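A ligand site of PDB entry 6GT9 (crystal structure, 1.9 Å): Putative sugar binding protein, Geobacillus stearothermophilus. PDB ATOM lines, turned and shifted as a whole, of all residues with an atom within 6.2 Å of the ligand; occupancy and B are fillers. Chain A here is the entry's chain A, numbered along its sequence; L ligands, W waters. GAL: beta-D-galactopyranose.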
ATOM      1  N   GLU A  38      26.986   4.051  -9.885  1.00  0.00           N
ATOM      2  CA  GLU A  38      26.755   5.201 -10.745  1.00  0.00           C
ATOM      3  C   GLU A  38      28.013   5.539 -11.552  1.00  0.00           C
ATOM      4  O   GLU A  38      27.927   5.921 -12.713  1.00  0.00           O
ATOM      5  CB  GLU A  38      26.315   6.406  -9.902  1.00  0.00           C
ATOM      6  CG  GLU A  38      25.894   7.653 -10.671  1.00  0.00           C
ATOM      7  CD  GLU A  38      25.245   8.684  -9.741  1.00  0.00           C
ATOM      8  OE1 GLU A  38      25.143   8.394  -8.536  1.00  0.00           O
ATOM      9  OE2 GLU A  38      24.846   9.775 -10.205  1.00  0.00           O
ATOM     10  N   ASN A  42      34.066   6.413  -8.318  1.00  0.00           N
ATOM     11  CA  ASN A  42      33.545   7.411  -7.379  1.00  0.00           C
ATOM     12  C   ASN A  42      33.778   6.940  -5.948  1.00  0.00           C
ATOM     13  O   ASN A  42      33.474   5.793  -5.612  1.00  0.00           O
ATOM     14  CB  ASN A  42      32.066   7.644  -7.630  1.00  0.00           C
ATOM     15  CG  ASN A  42      31.418   8.524  -6.545  1.00  0.00           C
ATOM     16  OD1 ASN A  42      30.878   8.022  -5.568  1.00  0.00           O
ATOM     17  ND2 ASN A  42      31.498   9.824  -6.721  1.00  0.00           N
ATOM     18  N   ASP A  43      34.272   7.831  -5.086  1.00  0.00           N
ATOM     19  CA  ASP A  43      34.690   7.415  -3.737  1.00  0.00           C
ATOM     20  C   ASP A  43      33.535   6.841  -2.921  1.00  0.00           C
ATOM     21  O   ASP A  43      33.733   5.910  -2.129  1.00  0.00           O
ATOM     22  CB  ASP A  43      35.299   8.592  -2.985  1.00  0.00           C
ATOM     23  CG  ASP A  43      36.674   8.981  -3.523  1.00  0.00           C
ATOM     24  OD1 ASP A  43      37.173   8.255  -4.418  1.00  0.00           O
ATOM     25  OD2 ASP A  43      37.239   9.982  -3.043  1.00  0.00           O
ATOM     26  N   TYR A  44      32.347   7.399  -3.061  1.00  0.00           N
ATOM     27  CA  TYR A  44      31.213   6.880  -2.301  1.00  0.00           C
ATOM     28  C   TYR A  44      30.846   5.472  -2.771  1.00  0.00           C
ATOM     29  O   TYR A  44      30.622   4.571  -1.953  1.00  0.00           O
ATOM     30  CB  TYR A  44      30.027   7.860  -2.432  1.00  0.00           C
ATOM     31  CG  TYR A  44      28.690   7.344  -1.909  1.00  0.00           C
ATOM     32  CD1 TYR A  44      27.880   6.547  -2.706  1.00  0.00           C
ATOM     33  CD2 TYR A  44      28.225   7.679  -0.626  1.00  0.00           C
ATOM     34  CE1 TYR A  44      26.654   6.074  -2.242  1.00  0.00           C
ATOM     35  CE2 TYR A  44      27.004   7.219  -0.162  1.00  0.00           C
ATOM     36  CZ  TYR A  44      26.221   6.405  -0.978  1.00  0.00           C
ATOM     37  OH  TYR A  44      25.000   5.932  -0.548  1.00  0.00           O
ATOM     38  N   TRP A  45      30.808   5.275  -4.094  1.00  0.00           N
ATOM     39  CA  TRP A  45      30.456   3.963  -4.628  1.00  0.00           C
ATOM     40  C   TRP A  45      31.507   2.898  -4.330  1.00  0.00           C
ATOM     41  O   TRP A  45      31.183   1.708  -4.236  1.00  0.00           O
ATOM     42  CB  TRP A  45      30.184   4.080  -6.135  1.00  0.00           C
ATOM     43  CG  TRP A  45      28.775   4.473  -6.301  1.00  0.00           C
ATOM     44  CD1 TRP A  45      28.294   5.715  -6.541  1.00  0.00           C
ATOM     45  CD2 TRP A  45      27.645   3.628  -6.107  1.00  0.00           C
ATOM     46  NE1 TRP A  45      26.921   5.702  -6.560  1.00  0.00           N
ATOM     47  CE2 TRP A  45      26.495   4.430  -6.287  1.00  0.00           C
ATOM     48  CE3 TRP A  45      27.490   2.262  -5.843  1.00  0.00           C
ATOM     49  CZ2 TRP A  45      25.210   3.912  -6.188  1.00  0.00           C
ATOM     50  CZ3 TRP A  45      26.205   1.751  -5.756  1.00  0.00           C
ATOM     51  CH2 TRP A  45      25.081   2.574  -5.938  1.00  0.00           C
ATOM     52  N   GLN A  94      21.307   1.166  -8.941  1.00  0.00           N
ATOM     53  CA  GLN A  94      20.385   2.277  -8.769  1.00  0.00           C
ATOM     54  C   GLN A  94      19.276   2.191  -9.802  1.00  0.00           C
ATOM     55  O   GLN A  94      19.496   1.762 -10.946  1.00  0.00           O
ATOM     56  CB  GLN A  94      21.104   3.609  -8.938  1.00  0.00           C
ATOM     57  CG  GLN A  94      22.095   3.995  -7.888  1.00  0.00           C
ATOM     58  CD  GLN A  94      23.063   5.022  -8.444  1.00  0.00           C
ATOM     59  OE1 GLN A  94      23.767   4.735  -9.403  1.00  0.00           O
ATOM     60  NE2 GLN A  94      23.062   6.239  -7.871  1.00  0.00           N
ATOM     61  N   ASP A 119      20.720   2.474  -3.095  1.00  0.00           N
ATOM     62  CA  ASP A 119      21.100   3.886  -3.039  1.00  0.00           C
ATOM     63  C   ASP A 119      20.043   4.799  -3.650  1.00  0.00           C
ATOM     64  O   ASP A 119      19.782   5.882  -3.128  1.00  0.00           O
ATOM     65  CB  ASP A 119      22.476   4.099  -3.719  1.00  0.00           C
ATOM     66  CG  ASP A 119      22.867   5.575  -3.849  1.00  0.00           C
ATOM     67  OD1 ASP A 119      22.521   6.186  -4.886  1.00  0.00           O
ATOM     68  OD2 ASP A 119      23.528   6.106  -2.930  1.00  0.00           O
ATOM     69  N   THR A 120      19.441   4.398  -4.761  1.00  0.00           N
ATOM     70  CA  THR A 120      18.387   5.139  -5.445  1.00  0.00           C
ATOM     71  C   THR A 120      17.329   4.125  -5.862  1.00  0.00           C
ATOM     72  O   THR A 120      17.654   3.146  -6.534  1.00  0.00           O
ATOM     73  CB  THR A 120      18.937   5.867  -6.687  1.00  0.00           C
ATOM     74  OG1 THR A 120      20.066   6.683  -6.331  1.00  0.00           O
ATOM     75  CG2 THR A 120      17.857   6.716  -7.360  1.00  0.00           C
ATOM     76  N   ASN A 135      15.523   9.088   0.188  1.00  0.00           N
ATOM     77  CA  ASN A 135      16.203  10.268  -0.364  1.00  0.00           C
ATOM     78  C   ASN A 135      15.375  11.541  -0.215  1.00  0.00           C
ATOM     79  O   ASN A 135      15.926  12.616   0.033  1.00  0.00           O
ATOM     80  CB  ASN A 135      16.569  10.000  -1.827  1.00  0.00           C
ATOM     81  CG  ASN A 135      17.734   9.076  -1.940  1.00  0.00           C
ATOM     82  OD1 ASN A 135      18.805   9.361  -1.396  1.00  0.00           O
ATOM     83  ND2 ASN A 135      17.542   7.943  -2.627  1.00  0.00           N
ATOM     84  N   HIS A 167      17.502  10.153  -7.160  1.00  0.00           N
ATOM     85  CA  HIS A 167      17.844  10.459  -5.767  1.00  0.00           C
ATOM     86  C   HIS A 167      18.215  11.924  -5.608  1.00  0.00           C
ATOM     87  O   HIS A 167      17.916  12.538  -4.573  1.00  0.00           O
ATOM     88  CB  HIS A 167      18.980   9.558  -5.254  1.00  0.00           C
ATOM     89  CG  HIS A 167      20.271   9.625  -6.027  1.00  0.00           C
ATOM     90  ND1 HIS A 167      20.325   9.864  -7.380  1.00  0.00           N
ATOM     91  CD2 HIS A 167      21.542   9.381  -5.640  1.00  0.00           C
ATOM     92  CE1 HIS A 167      21.582   9.801  -7.799  1.00  0.00           C
ATOM     93  NE2 HIS A 167      22.340   9.504  -6.756  1.00  0.00           N
ATOM     94  N   GLN A 168      18.856  12.502  -6.622  1.00  0.00           N
ATOM     95  CA  GLN A 168      19.153  13.932  -6.608  1.00  0.00           C
ATOM     96  C   GLN A 168      17.877  14.754  -6.645  1.00  0.00           C
ATOM     97  O   GLN A 168      17.735  15.721  -5.879  1.00  0.00           O
ATOM     98  CB  GLN A 168      20.063  14.273  -7.786  1.00  0.00           C
ATOM     99  CG  GLN A 168      21.385  13.532  -7.761  1.00  0.00           C
ATOM    100  CD  GLN A 168      22.154  13.819  -6.481  1.00  0.00           C
ATOM    101  OE1 GLN A 168      22.736  14.887  -6.322  1.00  0.00           O
ATOM    102  NE2 GLN A 168      22.130  12.868  -5.543  1.00  0.00           N
ATOM    103  N   ARG A 171      16.235  14.618  -3.160  1.00  0.00           N
ATOM    104  CA  ARG A 171      16.927  15.374  -2.124  1.00  0.00           C
ATOM    105  C   ARG A 171      16.757  16.882  -2.308  1.00  0.00           C
ATOM    106  O   ARG A 171      16.711  17.630  -1.318  1.00  0.00           O
ATOM    107  CB  ARG A 171      18.409  15.027  -2.093  1.00  0.00           C
ATOM    108  CG  ARG A 171      18.701  13.580  -1.727  1.00  0.00           C
ATOM    109  CD  ARG A 171      20.143  13.186  -2.052  1.00  0.00           C
ATOM    110  NE  ARG A 171      20.318  11.747  -1.915  1.00  0.00           N
ATOM    111  CZ  ARG A 171      21.461  11.096  -2.043  1.00  0.00           C
ATOM    112  NH1 ARG A 171      22.580  11.745  -2.335  1.00  0.00           N
ATOM    113  NH2 ARG A 171      21.471   9.771  -1.905  1.00  0.00           N
ATOM    114  N   ILE A 195      28.693  14.897 -10.378  1.00  0.00           N
ATOM    115  CA  ILE A 195      29.345  14.206  -9.262  1.00  0.00           C
ATOM    116  C   ILE A 195      30.876  14.215  -9.323  1.00  0.00           C
ATOM    117  O   ILE A 195      31.525  13.258  -8.887  1.00  0.00           O
ATOM    118  CB  ILE A 195      28.820  12.764  -9.107  1.00  0.00           C
ATOM    119  CG1 ILE A 195      29.169  11.857 -10.291  1.00  0.00           C
ATOM    120  CG2 ILE A 195      27.307  12.765  -8.884  1.00  0.00           C
ATOM    121  CD1 ILE A 195      28.868  10.408  -9.978  1.00  0.00           C
ATOM    122  N   THR A 220      23.994  18.044  -2.810  1.00  0.00           N
ATOM    123  CA  THR A 220      23.127  16.874  -2.650  1.00  0.00           C
ATOM    124  C   THR A 220      23.816  15.555  -2.972  1.00  0.00           C
ATOM    125  O   THR A 220      23.151  14.519  -2.952  1.00  0.00           O
ATOM    126  CB  THR A 220      21.866  17.012  -3.507  1.00  0.00           C
ATOM    127  OG1 THR A 220      22.193  16.961  -4.904  1.00  0.00           O
ATOM    128  CG2 THR A 220      21.164  18.338  -3.199  1.00  0.00           C
ATOM    129  N   SER A 221      25.110  15.565  -3.281  1.00  0.00           N
ATOM    130  CA  SER A 221      25.843  14.330  -3.510  1.00  0.00           C
ATOM    131  C   SER A 221      27.216  14.461  -2.868  1.00  0.00           C
ATOM    132  O   SER A 221      27.604  15.536  -2.407  1.00  0.00           O
ATOM    133  CB  SER A 221      25.921  13.999  -5.012  1.00  0.00           C
ATOM    134  OG  SER A 221      26.735  14.916  -5.724  1.00  0.00           O
ATOM    135  N   ALA A 222      27.979  13.358  -2.873  1.00  0.00           N
ATOM    136  CA  ALA A 222      29.045  13.182  -1.888  1.00  0.00           C
ATOM    137  C   ALA A 222      30.207  14.150  -2.050  1.00  0.00           C
ATOM    138  O   ALA A 222      30.921  14.394  -1.064  1.00  0.00           O
ATOM    139  CB  ALA A 222      29.573  11.753  -1.941  1.00  0.00           C
ATOM    140  N   LEU A 223      30.430  14.704  -3.235  1.00  0.00           N
ATOM    141  CA  LEU A 223      31.580  15.567  -3.485  1.00  0.00           C
ATOM    142  C   LEU A 223      31.201  17.039  -3.643  1.00  0.00           C
ATOM    143  O   LEU A 223      32.087  17.884  -3.805  1.00  0.00           O
ATOM    144  CB  LEU A 223      32.334  15.085  -4.742  1.00  0.00           C
ATOM    145  CG  LEU A 223      32.786  13.626  -4.648  1.00  0.00           C
ATOM    146  CD1 LEU A 223      33.306  13.099  -5.988  1.00  0.00           C
ATOM    147  CD2 LEU A 223      33.835  13.452  -3.561  1.00  0.00           C
ATOM    148  N   ASP A 224      29.908  17.364  -3.603  1.00  0.00           N
ATOM    149  CA  ASP A 224      29.469  18.721  -3.908  1.00  0.00           C
ATOM    150  C   ASP A 224      29.986  19.718  -2.881  1.00  0.00           C
ATOM    151  O   ASP A 224      30.558  20.757  -3.243  1.00  0.00           O
ATOM    152  CB  ASP A 224      27.950  18.766  -3.980  1.00  0.00           C
ATOM    153  CG  ASP A 224      27.415  17.955  -5.131  1.00  0.00           C
ATOM    154  OD1 ASP A 224      28.102  17.882  -6.161  1.00  0.00           O
ATOM    155  OD2 ASP A 224      26.293  17.419  -4.994  1.00  0.00           O
ATOM    156  N   PHE A 246      26.283  16.417   1.565  1.00  0.00           N
ATOM    157  CA  PHE A 246      25.904  15.024   1.760  1.00  0.00           C
ATOM    158  C   PHE A 246      27.136  14.165   2.024  1.00  0.00           C
ATOM    159  O   PHE A 246      28.227  14.440   1.525  1.00  0.00           O
ATOM    160  CB  PHE A 246      25.157  14.463   0.536  1.00  0.00           C
ATOM    161  CG  PHE A 246      23.667  14.326   0.752  1.00  0.00           C
ATOM    162  CD1 PHE A 246      22.855  15.447   0.766  1.00  0.00           C
ATOM    163  CD2 PHE A 246      23.101  13.079   0.967  1.00  0.00           C
ATOM    164  CE1 PHE A 246      21.494  15.331   0.968  1.00  0.00           C
ATOM    165  CE2 PHE A 246      21.740  12.954   1.181  1.00  0.00           C
ATOM    166  CZ  PHE A 246      20.933  14.097   1.183  1.00  0.00           C
ATOM    167  N   ASP A 247      26.920  13.132   2.840  1.00  0.00           N
ATOM    168  CA  ASP A 247      27.857  12.043   3.108  1.00  0.00           C
ATOM    169  C   ASP A 247      29.048  12.476   3.943  1.00  0.00           C
ATOM    170  O   ASP A 247      29.172  13.647   4.321  1.00  0.00           O
ATOM    171  CB  ASP A 247      28.313  11.396   1.795  1.00  0.00           C
ATOM    172  CG  ASP A 247      27.138  10.956   0.957  1.00  0.00           C
ATOM    173  OD1 ASP A 247      26.332  10.121   1.436  1.00  0.00           O
ATOM    174  OD2 ASP A 247      26.988  11.488  -0.141  1.00  0.00           O
ATOM    175  N   LEU A 249      32.566  11.495   3.531  1.00  0.00           N
ATOM    176  CA  LEU A 249      33.896  11.220   3.016  1.00  0.00           C
ATOM    177  C   LEU A 249      34.930  12.008   3.826  1.00  0.00           C
ATOM    178  O   LEU A 249      34.604  13.069   4.373  1.00  0.00           O
ATOM    179  CB  LEU A 249      33.992  11.592   1.533  1.00  0.00           C
ATOM    180  CG  LEU A 249      33.101  10.716   0.637  1.00  0.00           C
ATOM    181  CD1 LEU A 249      33.121  11.197  -0.801  1.00  0.00           C
ATOM    182  CD2 LEU A 249      33.514   9.241   0.719  1.00  0.00           C
ATOM    183  N   GLN A 267      24.793   9.051   5.212  1.00  0.00           N
ATOM    184  CA  GLN A 267      24.237   7.847   4.615  1.00  0.00           C
ATOM    185  C   GLN A 267      25.048   6.661   5.093  1.00  0.00           C
ATOM    186  O   GLN A 267      26.079   6.821   5.756  1.00  0.00           O
ATOM    187  CB  GLN A 267      24.226   7.906   3.080  1.00  0.00           C
ATOM    188  CG  GLN A 267      23.353   8.993   2.447  1.00  0.00           C
ATOM    189  CD  GLN A 267      23.184   8.784   0.957  1.00  0.00           C
ATOM    190  OE1 GLN A 267      22.217   8.168   0.512  1.00  0.00           O
ATOM    191  NE2 GLN A 267      24.156   9.252   0.173  1.00  0.00           N
ATOM    192  N   MET A 272      24.405  -0.430   2.847  1.00  0.00           N
ATOM    193  CA  MET A 272      23.494  -0.784   1.762  1.00  0.00           C
ATOM    194  C   MET A 272      24.123  -1.806   0.811  1.00  0.00           C
ATOM    195  O   MET A 272      23.413  -2.691   0.301  1.00  0.00           O
ATOM    196  CB  MET A 272      22.985   0.458   1.003  1.00  0.00           C
ATOM    197  CG  MET A 272      23.935   1.580   0.688  1.00  0.00           C
ATOM    198  SD  MET A 272      23.062   3.019  -0.034  1.00  0.00           S
ATOM    199  CE  MET A 272      23.011   4.201   1.321  1.00  0.00           C
HETATM  200  C1  GAL L   1      26.036  10.208  -3.009  1.00  0.00           C
HETATM  201  C2  GAL L   1      24.998   9.373  -3.748  1.00  0.00           C
HETATM  202  C3  GAL L   1      25.669   8.406  -4.746  1.00  0.00           C
HETATM  203  C4  GAL L   1      26.561   9.175  -5.707  1.00  0.00           C
HETATM  204  C5  GAL L   1      27.519  10.069  -4.941  1.00  0.00           C
HETATM  205  C6  GAL L   1      28.311  11.003  -5.856  1.00  0.00           C
HETATM  206  O1  GAL L   1      25.382  11.099  -2.130  1.00  0.00           O
HETATM  207  O2  GAL L   1      24.225   8.592  -2.832  1.00  0.00           O
HETATM  208  O3  GAL L   1      24.697   7.790  -5.531  1.00  0.00           O
HETATM  209  O4  GAL L   1      25.766   9.978  -6.585  1.00  0.00           O
HETATM  210  O5  GAL L   1      26.843  10.941  -3.948  1.00  0.00           O
HETATM  211  O6  GAL L   1      29.433  11.529  -5.192  1.00  0.00           O
HETATM  212  O   HOH W   1      29.211  14.167  -5.926  1.00  0.00           O
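The side-chain carboxylate (OD2) of Asp 119 is in hydrogen-bond range of an oxygen (O2) of the ligand (2.6 Å). An oxygen (O1) of the ligand sits at hydrogen-bond distance from the side-chain carboxylate of Asp 247 (2.6 Å). The side-chain carboxylate of Glu 38 is in hydrogen-bond range of an oxygen (O4) of the ligand (2.6 Å). The backbone NH of Ala 222 sits at hydrogen-bond distance from an oxygen (O5) of the ligand, 2.9 Å away. The guanidinium group (NH1) of Arg 171 lies within hydrogen-bond range of an oxygen (O1) of the ligand, at 2.9 Å. The side-chain amide nitrogen (NE2) of Gln 267 lies within hydrogen-bond range of an oxygen (O2) of the ligand (3.1 Å). The side-chain amide nitrogen of Asn 42 lies within hydrogen-bond range of an oxygen (O6) of the ligand. NE2 of His 167 lies within hydrogen-bond range of O3 of the ligand. The indole nitrogen (NE1) of Trp 45 is in hydrogen-bond range of an oxygen (O3) of the ligand, at 3.2 Å. The side-chain amide nitrogen (NE2) of Gln 94 is in hydrogen-bond range of an oxygen (O3) of the ligand (3.2 Å).
OH of Tyr 44 sits at hydrogen-bond distance from OD2 of Asp 119 (2.8 Å). The side-chain hydroxyl (OG1) of Thr 120 sits at hydrogen-bond distance from the side-chain carboxylate (OD1) of Asp 119 (2.9 Å). The side-chain carboxylate (OD2) of Asp 247 sits close to the backbone NH (N) of Ala 222 (3.5 Å). The side-chain amide nitrogen (NE2) of Gln 94 is in hydrogen-bond range of the side-chain carboxylate (OE1) of Glu 38 (3.1 Å). NH1 of Arg 171 lies close to NE2 of Gln 168 (3.4 Å). The guanidinium group of Arg 171 lies within hydrogen-bond range of the side-chain amide oxygen of Asn 135 (2.7 Å). The backbone NH of Tyr 44 is in hydrogen-bond range of the side-chain amide oxygen of Asn 42 (3.0 Å). The side-chain amide nitrogen of Gln 94 lies within hydrogen-bond range of the side-chain hydroxyl of Thr 120, 3.4 Å away.
Residues that only touch the ligand: Tyr 44 (3.5 Å), Ile 195 (3.6 Å), Ser 221 (3.4 Å) and Leu 223 (3.9 Å). Of the 23 residues printed, 14 come within 4 Å of the ligand. The nearest printed residue that does not touch the ligand is Thr 220 (4.2 Å).
Water W1 lies within hydrogen-bond range of the side-chain hydroxyl of Ser 221, an oxygen (O6) of the ligand, the backbone NH of Leu 223 and the backbone NH of Ala 222.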
